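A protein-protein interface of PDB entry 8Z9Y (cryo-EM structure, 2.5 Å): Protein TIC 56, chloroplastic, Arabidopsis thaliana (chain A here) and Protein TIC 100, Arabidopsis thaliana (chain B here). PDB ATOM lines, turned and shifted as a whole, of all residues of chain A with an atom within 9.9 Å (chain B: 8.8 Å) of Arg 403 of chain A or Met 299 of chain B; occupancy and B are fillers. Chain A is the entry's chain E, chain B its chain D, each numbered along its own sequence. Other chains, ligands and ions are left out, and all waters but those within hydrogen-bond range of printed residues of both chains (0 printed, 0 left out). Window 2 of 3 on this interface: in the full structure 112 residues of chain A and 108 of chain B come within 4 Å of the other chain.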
ATOM      1  N   MET A 382      -3.651  29.703 -26.977  1.00  0.00           N
ATOM      2  CA  MET A 382      -2.257  29.980 -26.682  1.00  0.00           C
ATOM      3  C   MET A 382      -1.607  30.697 -27.859  1.00  0.00           C
ATOM      4  O   MET A 382      -2.063  30.560 -28.998  1.00  0.00           O
ATOM      5  CB  MET A 382      -1.474  28.698 -26.372  1.00  0.00           C
ATOM      6  CG  MET A 382      -2.132  27.785 -25.365  1.00  0.00           C
ATOM      7  SD  MET A 382      -1.716  28.307 -23.692  1.00  0.00           S
ATOM      8  CE  MET A 382      -0.459  27.108 -23.266  1.00  0.00           C
ATOM      9  N   ILE A 387       6.483  28.326 -29.221  1.00  0.00           N
ATOM     10  CA  ILE A 387       6.292  26.913 -28.909  1.00  0.00           C
ATOM     11  C   ILE A 387       5.019  26.440 -29.601  1.00  0.00           C
ATOM     12  O   ILE A 387       3.933  26.503 -29.008  1.00  0.00           O
ATOM     13  CB  ILE A 387       6.230  26.672 -27.393  1.00  0.00           C
ATOM     14  CG1 ILE A 387       7.480  27.233 -26.713  1.00  0.00           C
ATOM     15  CG2 ILE A 387       6.087  25.186 -27.096  1.00  0.00           C
ATOM     16  CD1 ILE A 387       7.736  26.677 -25.331  1.00  0.00           C
ATOM     17  N   ARG A 392       4.963  21.581 -28.341  1.00  0.00           N
ATOM     18  CA  ARG A 392       4.399  21.455 -27.002  1.00  0.00           C
ATOM     19  C   ARG A 392       4.125  19.998 -26.655  1.00  0.00           C
ATOM     20  O   ARG A 392       4.376  19.563 -25.526  1.00  0.00           O
ATOM     21  CB  ARG A 392       3.121  22.284 -26.893  1.00  0.00           C
ATOM     22  CG  ARG A 392       2.570  22.383 -25.485  1.00  0.00           C
ATOM     23  CD  ARG A 392       1.066  22.200 -25.473  1.00  0.00           C
ATOM     24  NE  ARG A 392       0.394  23.176 -26.322  1.00  0.00           N
ATOM     25  CZ  ARG A 392      -0.920  23.259 -26.471  1.00  0.00           C
ATOM     26  NH1 ARG A 392      -1.740  22.436 -25.837  1.00  0.00           N
ATOM     27  NH2 ARG A 392      -1.425  24.192 -27.273  1.00  0.00           N
ATOM     28  N   LEU A 395       7.422  18.350 -25.901  1.00  0.00           N
ATOM     29  CA  LEU A 395       7.872  18.752 -24.573  1.00  0.00           C
ATOM     30  C   LEU A 395       7.100  18.016 -23.485  1.00  0.00           C
ATOM     31  O   LEU A 395       7.680  17.591 -22.480  1.00  0.00           O
ATOM     32  CB  LEU A 395       7.725  20.263 -24.404  1.00  0.00           C
ATOM     33  CG  LEU A 395       8.841  21.125 -24.996  1.00  0.00           C
ATOM     34  CD1 LEU A 395       8.408  22.579 -25.067  1.00  0.00           C
ATOM     35  CD2 LEU A 395      10.114  20.981 -24.182  1.00  0.00           C
ATOM     36  N   ALA A 396       5.787  17.859 -23.669  1.00  0.00           N
ATOM     37  CA  ALA A 396       4.987  17.104 -22.711  1.00  0.00           C
ATOM     38  C   ALA A 396       5.442  15.653 -22.640  1.00  0.00           C
ATOM     39  O   ALA A 396       5.429  15.041 -21.567  1.00  0.00           O
ATOM     40  CB  ALA A 396       3.506  17.185 -23.081  1.00  0.00           C
ATOM     41  N   ILE A 399       8.880  16.212 -20.712  1.00  0.00           N
ATOM     42  CA  ILE A 399       8.673  16.724 -19.361  1.00  0.00           C
ATOM     43  C   ILE A 399       7.333  16.189 -18.860  1.00  0.00           C
ATOM     44  O   ILE A 399       6.287  16.558 -19.417  1.00  0.00           O
ATOM     45  CB  ILE A 399       8.707  18.257 -19.326  1.00  0.00           C
ATOM     46  CG1 ILE A 399       9.988  18.774 -19.981  1.00  0.00           C
ATOM     47  CG2 ILE A 399       8.598  18.757 -17.897  1.00  0.00           C
ATOM     48  CD1 ILE A 399       9.970  20.256 -20.267  1.00  0.00           C
ATOM     49  N   PRO A 400       7.312  15.338 -17.830  1.00  0.00           N
ATOM     50  CA  PRO A 400       6.052  14.714 -17.403  1.00  0.00           C
ATOM     51  C   PRO A 400       4.978  15.703 -16.971  1.00  0.00           C
ATOM     52  O   PRO A 400       3.886  15.728 -17.547  1.00  0.00           O
ATOM     53  CB  PRO A 400       6.486  13.827 -16.226  1.00  0.00           C
ATOM     54  CG  PRO A 400       7.944  13.590 -16.447  1.00  0.00           C
ATOM     55  CD  PRO A 400       8.464  14.854 -17.053  1.00  0.00           C
ATOM     56  N   GLY A 401       5.273  16.520 -15.965  1.00  0.00           N
ATOM     57  CA  GLY A 401       4.280  17.429 -15.423  1.00  0.00           C
ATOM     58  C   GLY A 401       4.320  18.824 -16.011  1.00  0.00           C
ATOM     59  O   GLY A 401       4.518  19.801 -15.283  1.00  0.00           O
ATOM     60  N   LEU A 402       4.120  18.937 -17.320  1.00  0.00           N
ATOM     61  CA  LEU A 402       4.198  20.229 -17.991  1.00  0.00           C
ATOM     62  C   LEU A 402       2.873  20.968 -17.843  1.00  0.00           C
ATOM     63  O   LEU A 402       1.810  20.412 -18.136  1.00  0.00           O
ATOM     64  CB  LEU A 402       4.553  20.042 -19.463  1.00  0.00           C
ATOM     65  CG  LEU A 402       4.761  21.324 -20.271  1.00  0.00           C
ATOM     66  CD1 LEU A 402       6.129  21.917 -19.983  1.00  0.00           C
ATOM     67  CD2 LEU A 402       4.595  21.051 -21.754  1.00  0.00           C
ATOM     68  N   ARG A 403       2.938  22.221 -17.390  1.00  0.00           N
ATOM     69  CA  ARG A 403       1.768  23.065 -17.225  1.00  0.00           C
ATOM     70  C   ARG A 403       1.822  24.248 -18.189  1.00  0.00           C
ATOM     71  O   ARG A 403       2.906  24.678 -18.592  1.00  0.00           O
ATOM     72  CB  ARG A 403       1.663  23.582 -15.787  1.00  0.00           C
ATOM     73  CG  ARG A 403       2.158  22.602 -14.740  1.00  0.00           C
ATOM     74  CD  ARG A 403       1.001  21.910 -14.043  1.00  0.00           C
ATOM     75  NE  ARG A 403      -0.079  22.835 -13.726  1.00  0.00           N
ATOM     76  CZ  ARG A 403      -1.265  22.470 -13.258  1.00  0.00           C
ATOM     77  NH1 ARG A 403      -1.558  21.199 -13.039  1.00  0.00           N
ATOM     78  NH2 ARG A 403      -2.178  23.403 -13.005  1.00  0.00           N
ATOM     79  N   PRO A 404       0.666  24.790 -18.584  1.00  0.00           N
ATOM     80  CA  PRO A 404       0.665  25.867 -19.589  1.00  0.00           C
ATOM     81  C   PRO A 404       1.415  27.121 -19.170  1.00  0.00           C
ATOM     82  O   PRO A 404       1.918  27.848 -20.038  1.00  0.00           O
ATOM     83  CB  PRO A 404      -0.831  26.151 -19.787  1.00  0.00           C
ATOM     84  CG  PRO A 404      -1.511  24.894 -19.375  1.00  0.00           C
ATOM     85  CD  PRO A 404      -0.699  24.356 -18.242  1.00  0.00           C
ATOM     86  N   TRP A 405       1.500  27.406 -17.868  1.00  0.00           N
ATOM     87  CA  TRP A 405       2.116  28.657 -17.440  1.00  0.00           C
ATOM     88  C   TRP A 405       3.605  28.691 -17.756  1.00  0.00           C
ATOM     89  O   TRP A 405       4.152  29.765 -18.018  1.00  0.00           O
ATOM     90  CB  TRP A 405       1.872  28.891 -15.948  1.00  0.00           C
ATOM     91  CG  TRP A 405       2.577  27.940 -15.039  1.00  0.00           C
ATOM     92  CD1 TRP A 405       2.112  26.744 -14.585  1.00  0.00           C
ATOM     93  CD2 TRP A 405       3.869  28.118 -14.447  1.00  0.00           C
ATOM     94  NE1 TRP A 405       3.037  26.158 -13.759  1.00  0.00           N
ATOM     95  CE2 TRP A 405       4.126  26.982 -13.657  1.00  0.00           C
ATOM     96  CE3 TRP A 405       4.837  29.124 -14.514  1.00  0.00           C
ATOM     97  CZ2 TRP A 405       5.307  26.824 -12.938  1.00  0.00           C
ATOM     98  CZ3 TRP A 405       6.009  28.966 -13.801  1.00  0.00           C
ATOM     99  CH2 TRP A 405       6.235  27.824 -13.023  1.00  0.00           C
ATOM    100  N   GLU A 406       4.273  27.536 -17.751  1.00  0.00           N
ATOM    101  CA  GLU A 406       5.680  27.503 -18.141  1.00  0.00           C
ATOM    102  C   GLU A 406       5.856  27.888 -19.605  1.00  0.00           C
ATOM    103  O   GLU A 406       6.757  28.663 -19.952  1.00  0.00           O
ATOM    104  CB  GLU A 406       6.260  26.116 -17.874  1.00  0.00           C
ATOM    105  CG  GLU A 406       6.341  25.760 -16.402  1.00  0.00           C
ATOM    106  CD  GLU A 406       6.238  24.269 -16.160  1.00  0.00           C
ATOM    107  OE1 GLU A 406       5.903  23.534 -17.110  1.00  0.00           O
ATOM    108  OE2 GLU A 406       6.489  23.832 -15.017  1.00  0.00           O
ATOM    109  N   VAL A 407       4.995  27.362 -20.480  1.00  0.00           N
ATOM    110  CA  VAL A 407       5.048  27.724 -21.893  1.00  0.00           C
ATOM    111  C   VAL A 407       4.759  29.207 -22.074  1.00  0.00           C
ATOM    112  O   VAL A 407       5.411  29.893 -22.874  1.00  0.00           O
ATOM    113  CB  VAL A 407       4.068  26.854 -22.702  1.00  0.00           C
ATOM    114  CG1 VAL A 407       4.231  27.112 -24.190  1.00  0.00           C
ATOM    115  CG2 VAL A 407       4.283  25.385 -22.386  1.00  0.00           C
ATOM    116  N   ILE A 408       3.774  29.727 -21.336  1.00  0.00           N
ATOM    117  CA  ILE A 408       3.447  31.147 -21.430  1.00  0.00           C
ATOM    118  C   ILE A 408       4.631  31.998 -20.987  1.00  0.00           C
ATOM    119  O   ILE A 408       4.955  33.011 -21.616  1.00  0.00           O
ATOM    120  CB  ILE A 408       2.182  31.458 -20.610  1.00  0.00           C
ATOM    121  CG1 ILE A 408       0.951  30.857 -21.287  1.00  0.00           C
ATOM    122  CG2 ILE A 408       2.007  32.957 -20.437  1.00  0.00           C
ATOM    123  CD1 ILE A 408      -0.248  30.739 -20.376  1.00  0.00           C
ATOM    124  N   SER A 409       5.293  31.604 -19.897  1.00  0.00           N
ATOM    125  CA  SER A 409       6.449  32.351 -19.413  1.00  0.00           C
ATOM    126  C   SER A 409       7.587  32.328 -20.424  1.00  0.00           C
ATOM    127  O   SER A 409       8.255  33.347 -20.639  1.00  0.00           O
ATOM    128  CB  SER A 409       6.911  31.784 -18.071  1.00  0.00           C
ATOM    129  OG  SER A 409       8.195  32.272 -17.730  1.00  0.00           O
ATOM    130  N   ILE A 410       7.835  31.172 -21.044  1.00  0.00           N
ATOM    131  CA  ILE A 410       8.883  31.090 -22.058  1.00  0.00           C
ATOM    132  C   ILE A 410       8.554  31.997 -23.237  1.00  0.00           C
ATOM    133  O   ILE A 410       9.427  32.703 -23.761  1.00  0.00           O
ATOM    134  CB  ILE A 410       9.087  29.630 -22.502  1.00  0.00           C
ATOM    135  CG1 ILE A 410       9.684  28.805 -21.362  1.00  0.00           C
ATOM    136  CG2 ILE A 410       9.979  29.563 -23.730  1.00  0.00           C
ATOM    137  CD1 ILE A 410      11.136  29.109 -21.083  1.00  0.00           C
ATOM    138  N   PRO B 269     -14.429  25.072 -14.420  1.00  0.00           N
ATOM    139  CA  PRO B 269     -14.554  23.613 -14.320  1.00  0.00           C
ATOM    140  C   PRO B 269     -14.540  23.138 -12.875  1.00  0.00           C
ATOM    141  O   PRO B 269     -13.779  23.638 -12.042  1.00  0.00           O
ATOM    142  CB  PRO B 269     -13.332  23.100 -15.090  1.00  0.00           C
ATOM    143  CG  PRO B 269     -12.982  24.210 -16.023  1.00  0.00           C
ATOM    144  CD  PRO B 269     -13.309  25.475 -15.287  1.00  0.00           C
ATOM    145  N   ARG B 286     -16.635  23.422 -23.347  1.00  0.00           N
ATOM    146  CA  ARG B 286     -15.503  22.522 -23.167  1.00  0.00           C
ATOM    147  C   ARG B 286     -15.874  21.055 -23.343  1.00  0.00           C
ATOM    148  O   ARG B 286     -14.972  20.212 -23.397  1.00  0.00           O
ATOM    149  CB  ARG B 286     -14.873  22.738 -21.789  1.00  0.00           C
ATOM    150  CG  ARG B 286     -15.552  21.988 -20.659  1.00  0.00           C
ATOM    151  CD  ARG B 286     -14.831  22.231 -19.344  1.00  0.00           C
ATOM    152  NE  ARG B 286     -15.465  21.535 -18.231  1.00  0.00           N
ATOM    153  CZ  ARG B 286     -15.121  20.326 -17.811  1.00  0.00           C
ATOM    154  NH1 ARG B 286     -14.144  19.646 -18.389  1.00  0.00           N
ATOM    155  NH2 ARG B 286     -15.771  19.786 -16.785  1.00  0.00           N
ATOM    156  N   PRO B 291     -10.051  15.245 -25.621  1.00  0.00           N
ATOM    157  CA  PRO B 291      -9.707  15.163 -24.190  1.00  0.00           C
ATOM    158  C   PRO B 291      -8.403  15.850 -23.827  1.00  0.00           C
ATOM    159  O   PRO B 291      -8.308  16.453 -22.749  1.00  0.00           O
ATOM    160  CB  PRO B 291      -9.641  13.650 -23.941  1.00  0.00           C
ATOM    161  CG  PRO B 291     -10.532  13.062 -24.981  1.00  0.00           C
ATOM    162  CD  PRO B 291     -10.353  13.923 -26.196  1.00  0.00           C
ATOM    163  N   GLU B 292      -7.392  15.780 -24.694  1.00  0.00           N
ATOM    164  CA  GLU B 292      -6.125  16.443 -24.401  1.00  0.00           C
ATOM    165  C   GLU B 292      -6.308  17.952 -24.302  1.00  0.00           C
ATOM    166  O   GLU B 292      -5.806  18.592 -23.371  1.00  0.00           O
ATOM    167  CB  GLU B 292      -5.086  16.088 -25.467  1.00  0.00           C
ATOM    168  CG  GLU B 292      -5.593  16.180 -26.900  1.00  0.00           C
ATOM    169  CD  GLU B 292      -6.134  14.861 -27.417  1.00  0.00           C
ATOM    170  OE1 GLU B 292      -6.369  13.950 -26.597  1.00  0.00           O
ATOM    171  OE2 GLU B 292      -6.325  14.738 -28.645  1.00  0.00           O
ATOM    172  N   ASP B 293      -7.045  18.537 -25.250  1.00  0.00           N
ATOM    173  CA  ASP B 293      -7.295  19.974 -25.211  1.00  0.00           C
ATOM    174  C   ASP B 293      -8.131  20.357 -23.998  1.00  0.00           C
ATOM    175  O   ASP B 293      -7.902  21.407 -23.389  1.00  0.00           O
ATOM    176  CB  ASP B 293      -7.980  20.425 -26.499  1.00  0.00           C
ATOM    177  CG  ASP B 293      -7.177  20.082 -27.736  1.00  0.00           C
ATOM    178  OD1 ASP B 293      -5.945  20.284 -27.719  1.00  0.00           O
ATOM    179  OD2 ASP B 293      -7.776  19.615 -28.727  1.00  0.00           O
ATOM    180  N   ARG B 294      -9.111  19.526 -23.639  1.00  0.00           N
ATOM    181  CA  ARG B 294      -9.933  19.818 -22.469  1.00  0.00           C
ATOM    182  C   ARG B 294      -9.100  19.815 -21.192  1.00  0.00           C
ATOM    183  O   ARG B 294      -9.228  20.719 -20.357  1.00  0.00           O
ATOM    184  CB  ARG B 294     -11.076  18.809 -22.375  1.00  0.00           C
ATOM    185  CG  ARG B 294     -11.744  18.740 -21.015  1.00  0.00           C
ATOM    186  CD  ARG B 294     -12.795  17.647 -20.990  1.00  0.00           C
ATOM    187  NE  ARG B 294     -13.460  17.514 -22.280  1.00  0.00           N
ATOM    188  CZ  ARG B 294     -13.735  16.356 -22.865  1.00  0.00           C
ATOM    189  NH1 ARG B 294     -13.414  15.204 -22.301  1.00  0.00           N
ATOM    190  NH2 ARG B 294     -14.345  16.356 -24.046  1.00  0.00           N
ATOM    191  N   LYS B 295      -8.231  18.813 -21.029  1.00  0.00           N
ATOM    192  CA  LYS B 295      -7.368  18.771 -19.853  1.00  0.00           C
ATOM    193  C   LYS B 295      -6.402  19.949 -19.837  1.00  0.00           C
ATOM    194  O   LYS B 295      -6.148  20.548 -18.781  1.00  0.00           O
ATOM    195  CB  LYS B 295      -6.608  17.444 -19.816  1.00  0.00           C
ATOM    196  CG  LYS B 295      -5.423  17.425 -18.869  1.00  0.00           C
ATOM    197  CD  LYS B 295      -5.403  16.146 -18.049  1.00  0.00           C
ATOM    198  CE  LYS B 295      -4.442  16.253 -16.877  1.00  0.00           C
ATOM    199  NZ  LYS B 295      -4.959  17.157 -15.813  1.00  0.00           N
ATOM    200  N   TRP B 296      -5.855  20.298 -21.005  1.00  0.00           N
ATOM    201  CA  TRP B 296      -4.958  21.443 -21.097  1.00  0.00           C
ATOM    202  C   TRP B 296      -5.666  22.728 -20.683  1.00  0.00           C
ATOM    203  O   TRP B 296      -5.106  23.541 -19.938  1.00  0.00           O
ATOM    204  CB  TRP B 296      -4.423  21.556 -22.524  1.00  0.00           C
ATOM    205  CG  TRP B 296      -3.305  22.526 -22.684  1.00  0.00           C
ATOM    206  CD1 TRP B 296      -3.369  23.761 -23.252  1.00  0.00           C
ATOM    207  CD2 TRP B 296      -1.943  22.336 -22.286  1.00  0.00           C
ATOM    208  NE1 TRP B 296      -2.134  24.358 -23.226  1.00  0.00           N
ATOM    209  CE2 TRP B 296      -1.240  23.503 -22.638  1.00  0.00           C
ATOM    210  CE3 TRP B 296      -1.251  21.294 -21.664  1.00  0.00           C
ATOM    211  CZ2 TRP B 296       0.120  23.658 -22.389  1.00  0.00           C
ATOM    212  CZ3 TRP B 296       0.099  21.450 -21.417  1.00  0.00           C
ATOM    213  CH2 TRP B 296       0.770  22.622 -21.779  1.00  0.00           C
ATOM    214  N   LEU B 297      -6.901  22.923 -21.148  1.00  0.00           N
ATOM    215  CA  LEU B 297      -7.656  24.115 -20.778  1.00  0.00           C
ATOM    216  C   LEU B 297      -7.987  24.120 -19.291  1.00  0.00           C
ATOM    217  O   LEU B 297      -7.976  25.179 -18.654  1.00  0.00           O
ATOM    218  CB  LEU B 297      -8.932  24.215 -21.612  1.00  0.00           C
ATOM    219  CG  LEU B 297      -9.904  25.316 -21.184  1.00  0.00           C
ATOM    220  CD1 LEU B 297      -9.282  26.688 -21.388  1.00  0.00           C
ATOM    221  CD2 LEU B 297     -11.219  25.209 -21.932  1.00  0.00           C
ATOM    222  N   GLU B 298      -8.299  22.954 -18.722  1.00  0.00           N
ATOM    223  CA  GLU B 298      -8.564  22.888 -17.288  1.00  0.00           C
ATOM    224  C   GLU B 298      -7.339  23.316 -16.490  1.00  0.00           C
ATOM    225  O   GLU B 298      -7.443  24.100 -15.535  1.00  0.00           O
ATOM    226  CB  GLU B 298      -8.995  21.475 -16.898  1.00  0.00           C
ATOM    227  CG  GLU B 298     -10.376  21.088 -17.393  1.00  0.00           C
ATOM    228  CD  GLU B 298     -10.748  19.666 -17.023  1.00  0.00           C
ATOM    229  OE1 GLU B 298     -10.073  19.084 -16.149  1.00  0.00           O
ATOM    230  OE2 GLU B 298     -11.715  19.132 -17.605  1.00  0.00           O
ATOM    231  N   MET B 299      -6.163  22.818 -16.876  1.00  0.00           N
ATOM    232  CA  MET B 299      -4.937  23.223 -16.193  1.00  0.00           C
ATOM    233  C   MET B 299      -4.666  24.711 -16.384  1.00  0.00           C
ATOM    234  O   MET B 299      -4.212  25.392 -15.456  1.00  0.00           O
ATOM    235  CB  MET B 299      -3.758  22.386 -16.687  1.00  0.00           C
ATOM    236  CG  MET B 299      -3.585  21.075 -15.939  1.00  0.00           C
ATOM    237  SD  MET B 299      -2.257  20.041 -16.584  1.00  0.00           S
ATOM    238  CE  MET B 299      -2.166  20.610 -18.278  1.00  0.00           C
ATOM    239  N   ASP B 300      -4.938  25.233 -17.582  1.00  0.00           N
ATOM    240  CA  ASP B 300      -4.747  26.658 -17.836  1.00  0.00           C
ATOM    241  C   ASP B 300      -5.640  27.505 -16.938  1.00  0.00           C
ATOM    242  O   ASP B 300      -5.196  28.516 -16.380  1.00  0.00           O
ATOM    243  CB  ASP B 300      -5.023  26.964 -19.307  1.00  0.00           C
ATOM    244  CG  ASP B 300      -4.367  28.248 -19.771  1.00  0.00           C
ATOM    245  OD1 ASP B 300      -3.850  28.999 -18.919  1.00  0.00           O
ATOM    246  OD2 ASP B 300      -4.371  28.506 -20.993  1.00  0.00           O
ATOM    247  N   VAL B 301      -6.905  27.111 -16.789  1.00  0.00           N
ATOM    248  CA  VAL B 301      -7.828  27.869 -15.951  1.00  0.00           C
ATOM    249  C   VAL B 301      -7.418  27.776 -14.487  1.00  0.00           C
ATOM    250  O   VAL B 301      -7.508  28.760 -13.742  1.00  0.00           O
ATOM    251  CB  VAL B 301      -9.273  27.388 -16.173  1.00  0.00           C
ATOM    252  CG1 VAL B 301     -10.221  28.089 -15.217  1.00  0.00           C
ATOM    253  CG2 VAL B 301      -9.693  27.642 -17.607  1.00  0.00           C
ATOM    254  N   GLU B 302      -6.954  26.602 -14.052  1.00  0.00           N
ATOM    255  CA  GLU B 302      -6.460  26.474 -12.684  1.00  0.00           C
ATOM    256  C   GLU B 302      -5.274  27.401 -12.440  1.00  0.00           C
ATOM    257  O   GLU B 302      -5.205  28.078 -11.405  1.00  0.00           O
ATOM    258  CB  GLU B 302      -6.069  25.025 -12.402  1.00  0.00           C
ATOM    259  CG  GLU B 302      -7.179  24.182 -11.809  1.00  0.00           C
ATOM    260  CD  GLU B 302      -6.675  22.854 -11.282  1.00  0.00           C
ATOM    261  OE1 GLU B 302      -5.745  22.859 -10.449  1.00  0.00           O
ATOM    262  OE2 GLU B 302      -7.204  21.805 -11.706  1.00  0.00           O
ATOM    263  N   ASP B 303      -4.337  27.449 -13.389  1.00  0.00           N
ATOM    264  CA  ASP B 303      -3.181  28.330 -13.250  1.00  0.00           C
ATOM    265  C   ASP B 303      -3.599  29.793 -13.219  1.00  0.00           C
ATOM    266  O   ASP B 303      -3.068  30.580 -12.428  1.00  0.00           O
ATOM    267  CB  ASP B 303      -2.192  28.080 -14.387  1.00  0.00           C
ATOM    268  CG  ASP B 303      -1.468  26.759 -14.248  1.00  0.00           C
ATOM    269  OD1 ASP B 303      -1.494  26.178 -13.142  1.00  0.00           O
ATOM    270  OD2 ASP B 303      -0.874  26.299 -15.245  1.00  0.00           O
ATOM    271  N   SER B 304      -4.542  30.180 -14.082  1.00  0.00           N
ATOM    272  CA  SER B 304      -5.007  31.563 -14.098  1.00  0.00           C
ATOM    273  C   SER B 304      -5.673  31.937 -12.781  1.00  0.00           C
ATOM    274  O   SER B 304      -5.443  33.031 -12.250  1.00  0.00           O
ATOM    275  CB  SER B 304      -5.969  31.780 -15.265  1.00  0.00           C
ATOM    276  OG  SER B 304      -5.268  31.867 -16.493  1.00  0.00           O
ATOM    277  N   VAL B 305      -6.499  31.041 -12.237  1.00  0.00           N
ATOM    278  CA  VAL B 305      -7.160  31.316 -10.965  1.00  0.00           C
ATOM    279  C   VAL B 305      -6.133  31.445  -9.848  1.00  0.00           C
ATOM    280  O   VAL B 305      -6.226  32.340  -8.999  1.00  0.00           O
ATOM    281  CB  VAL B 305      -8.203  30.226 -10.656  1.00  0.00           C
ATOM    282  CG1 VAL B 305      -8.634  30.297  -9.201  1.00  0.00           C
ATOM    283  CG2 VAL B 305      -9.403  30.369 -11.575  1.00  0.00           C
ATOM    284  N   ALA B 306      -5.136  30.556  -9.829  1.00  0.00           N
ATOM    285  CA  ALA B 306      -4.102  30.635  -8.802  1.00  0.00           C
ATOM    286  C   ALA B 306      -3.309  31.931  -8.911  1.00  0.00           C
ATOM    287  O   ALA B 306      -2.993  32.562  -7.896  1.00  0.00           O
ATOM    288  CB  ALA B 306      -3.172  29.426  -8.898  1.00  0.00           C
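Among the printed residues, pairs that only touch across the chains: Trp 405 of chain A with Asp 303 of chain B (3.1 Å), Met 382 of chain A with Trp 296 of chain B (3.2 Å), Pro 404 of chain A with Trp 296 of chain B (3.6 Å), Pro 404 of chain A with Asp 303 of chain B (3.6 Å), Leu 402 of chain A with Trp 296 of chain B (3.8 Å), Pro 404 of chain A with Asp 300 of chain B (3.9 Å), Pro 404 of chain A with Met 299 of chain B (3.96 Å) and Leu 402 of chain A with Met 299 of chain B (3.98 Å).
Printed residues of chain B within 4 Å of Met 382 of chain A: Trp 296 and Asp 300. Printed residues of chain B within 4 Å of Arg 392 of chain A: Trp 296 (3.3 Å). Arg 403 of chain A touches two residues of chain B. Of chain B, only Trp 296, Met 299, Asp 300 and Asp 303 come within 4 Å of Pro 404 of chain A. Printed residues of chain A within 4 Å of Met 299 of chain B: Leu 402 (3.98 Å), Arg 403 (3.5 Å) and Pro 404 (3.96 Å). Printed residues of chain A within 4 Å of Asp 300 of chain B: Met 382 and Pro 404. No residue of chain A comes within 4 Å of Glu 302 of chain B. Of the printed residues of chain A, Asp 303 of chain B touches Arg 403, Pro 404 and Trp 405. The nearest residue of chain B that does not touch Arg 403 of chain A is Trp 296 of chain B (4.1 Å).
The side-chain carboxylate (OE1) of Glu 406 of chain A is in hydrogen-bond range of the backbone NH (N) of Arg 403 of chain A, 3.3 Å away. O of Asp 300 of chain B sits at hydrogen-bond distance from OG of Ser 304 of chain B (3.4 Å).
Of the 18 printed residues of chain B, 4 touch a printed residue of chain A. Printed residues of chain B that touch a printed residue of chain A: Trp 296, Met 299, Asp 300 and Asp 303. Of the 17 printed residues of chain A, 6 touch a printed residue of chain B. Hydrophobic or aromatic side chains of chain A within 4 Å of the printed part of chain B: Met 382, Pro 404 and Trp 405. Along chain A the printed residues that touch a printed residue of chain B span positions 382 to 405.
The guanidinium group (NH2) of Arg 403 of chain A is in salt-bridge range of the side-chain carboxylate (OD1) of Asp 303 of chain B, at 2.9 Å. The indole nitrogen (NE1) of Trp 296 of chain B sits close to the guanidinium group (NH1) of Arg 392 of chain A (3.3 Å). The side-chain sulfur (SD) of Met 382 of chain A sits close to the side-chain carboxylate (OD2) of Asp 300 of chain B (3.8 Å). The guanidinium group (NH1) of Arg 403 of chain A lies close to the side-chain sulfur (SD) of Met 299 of chain B, 3.8 Å away.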
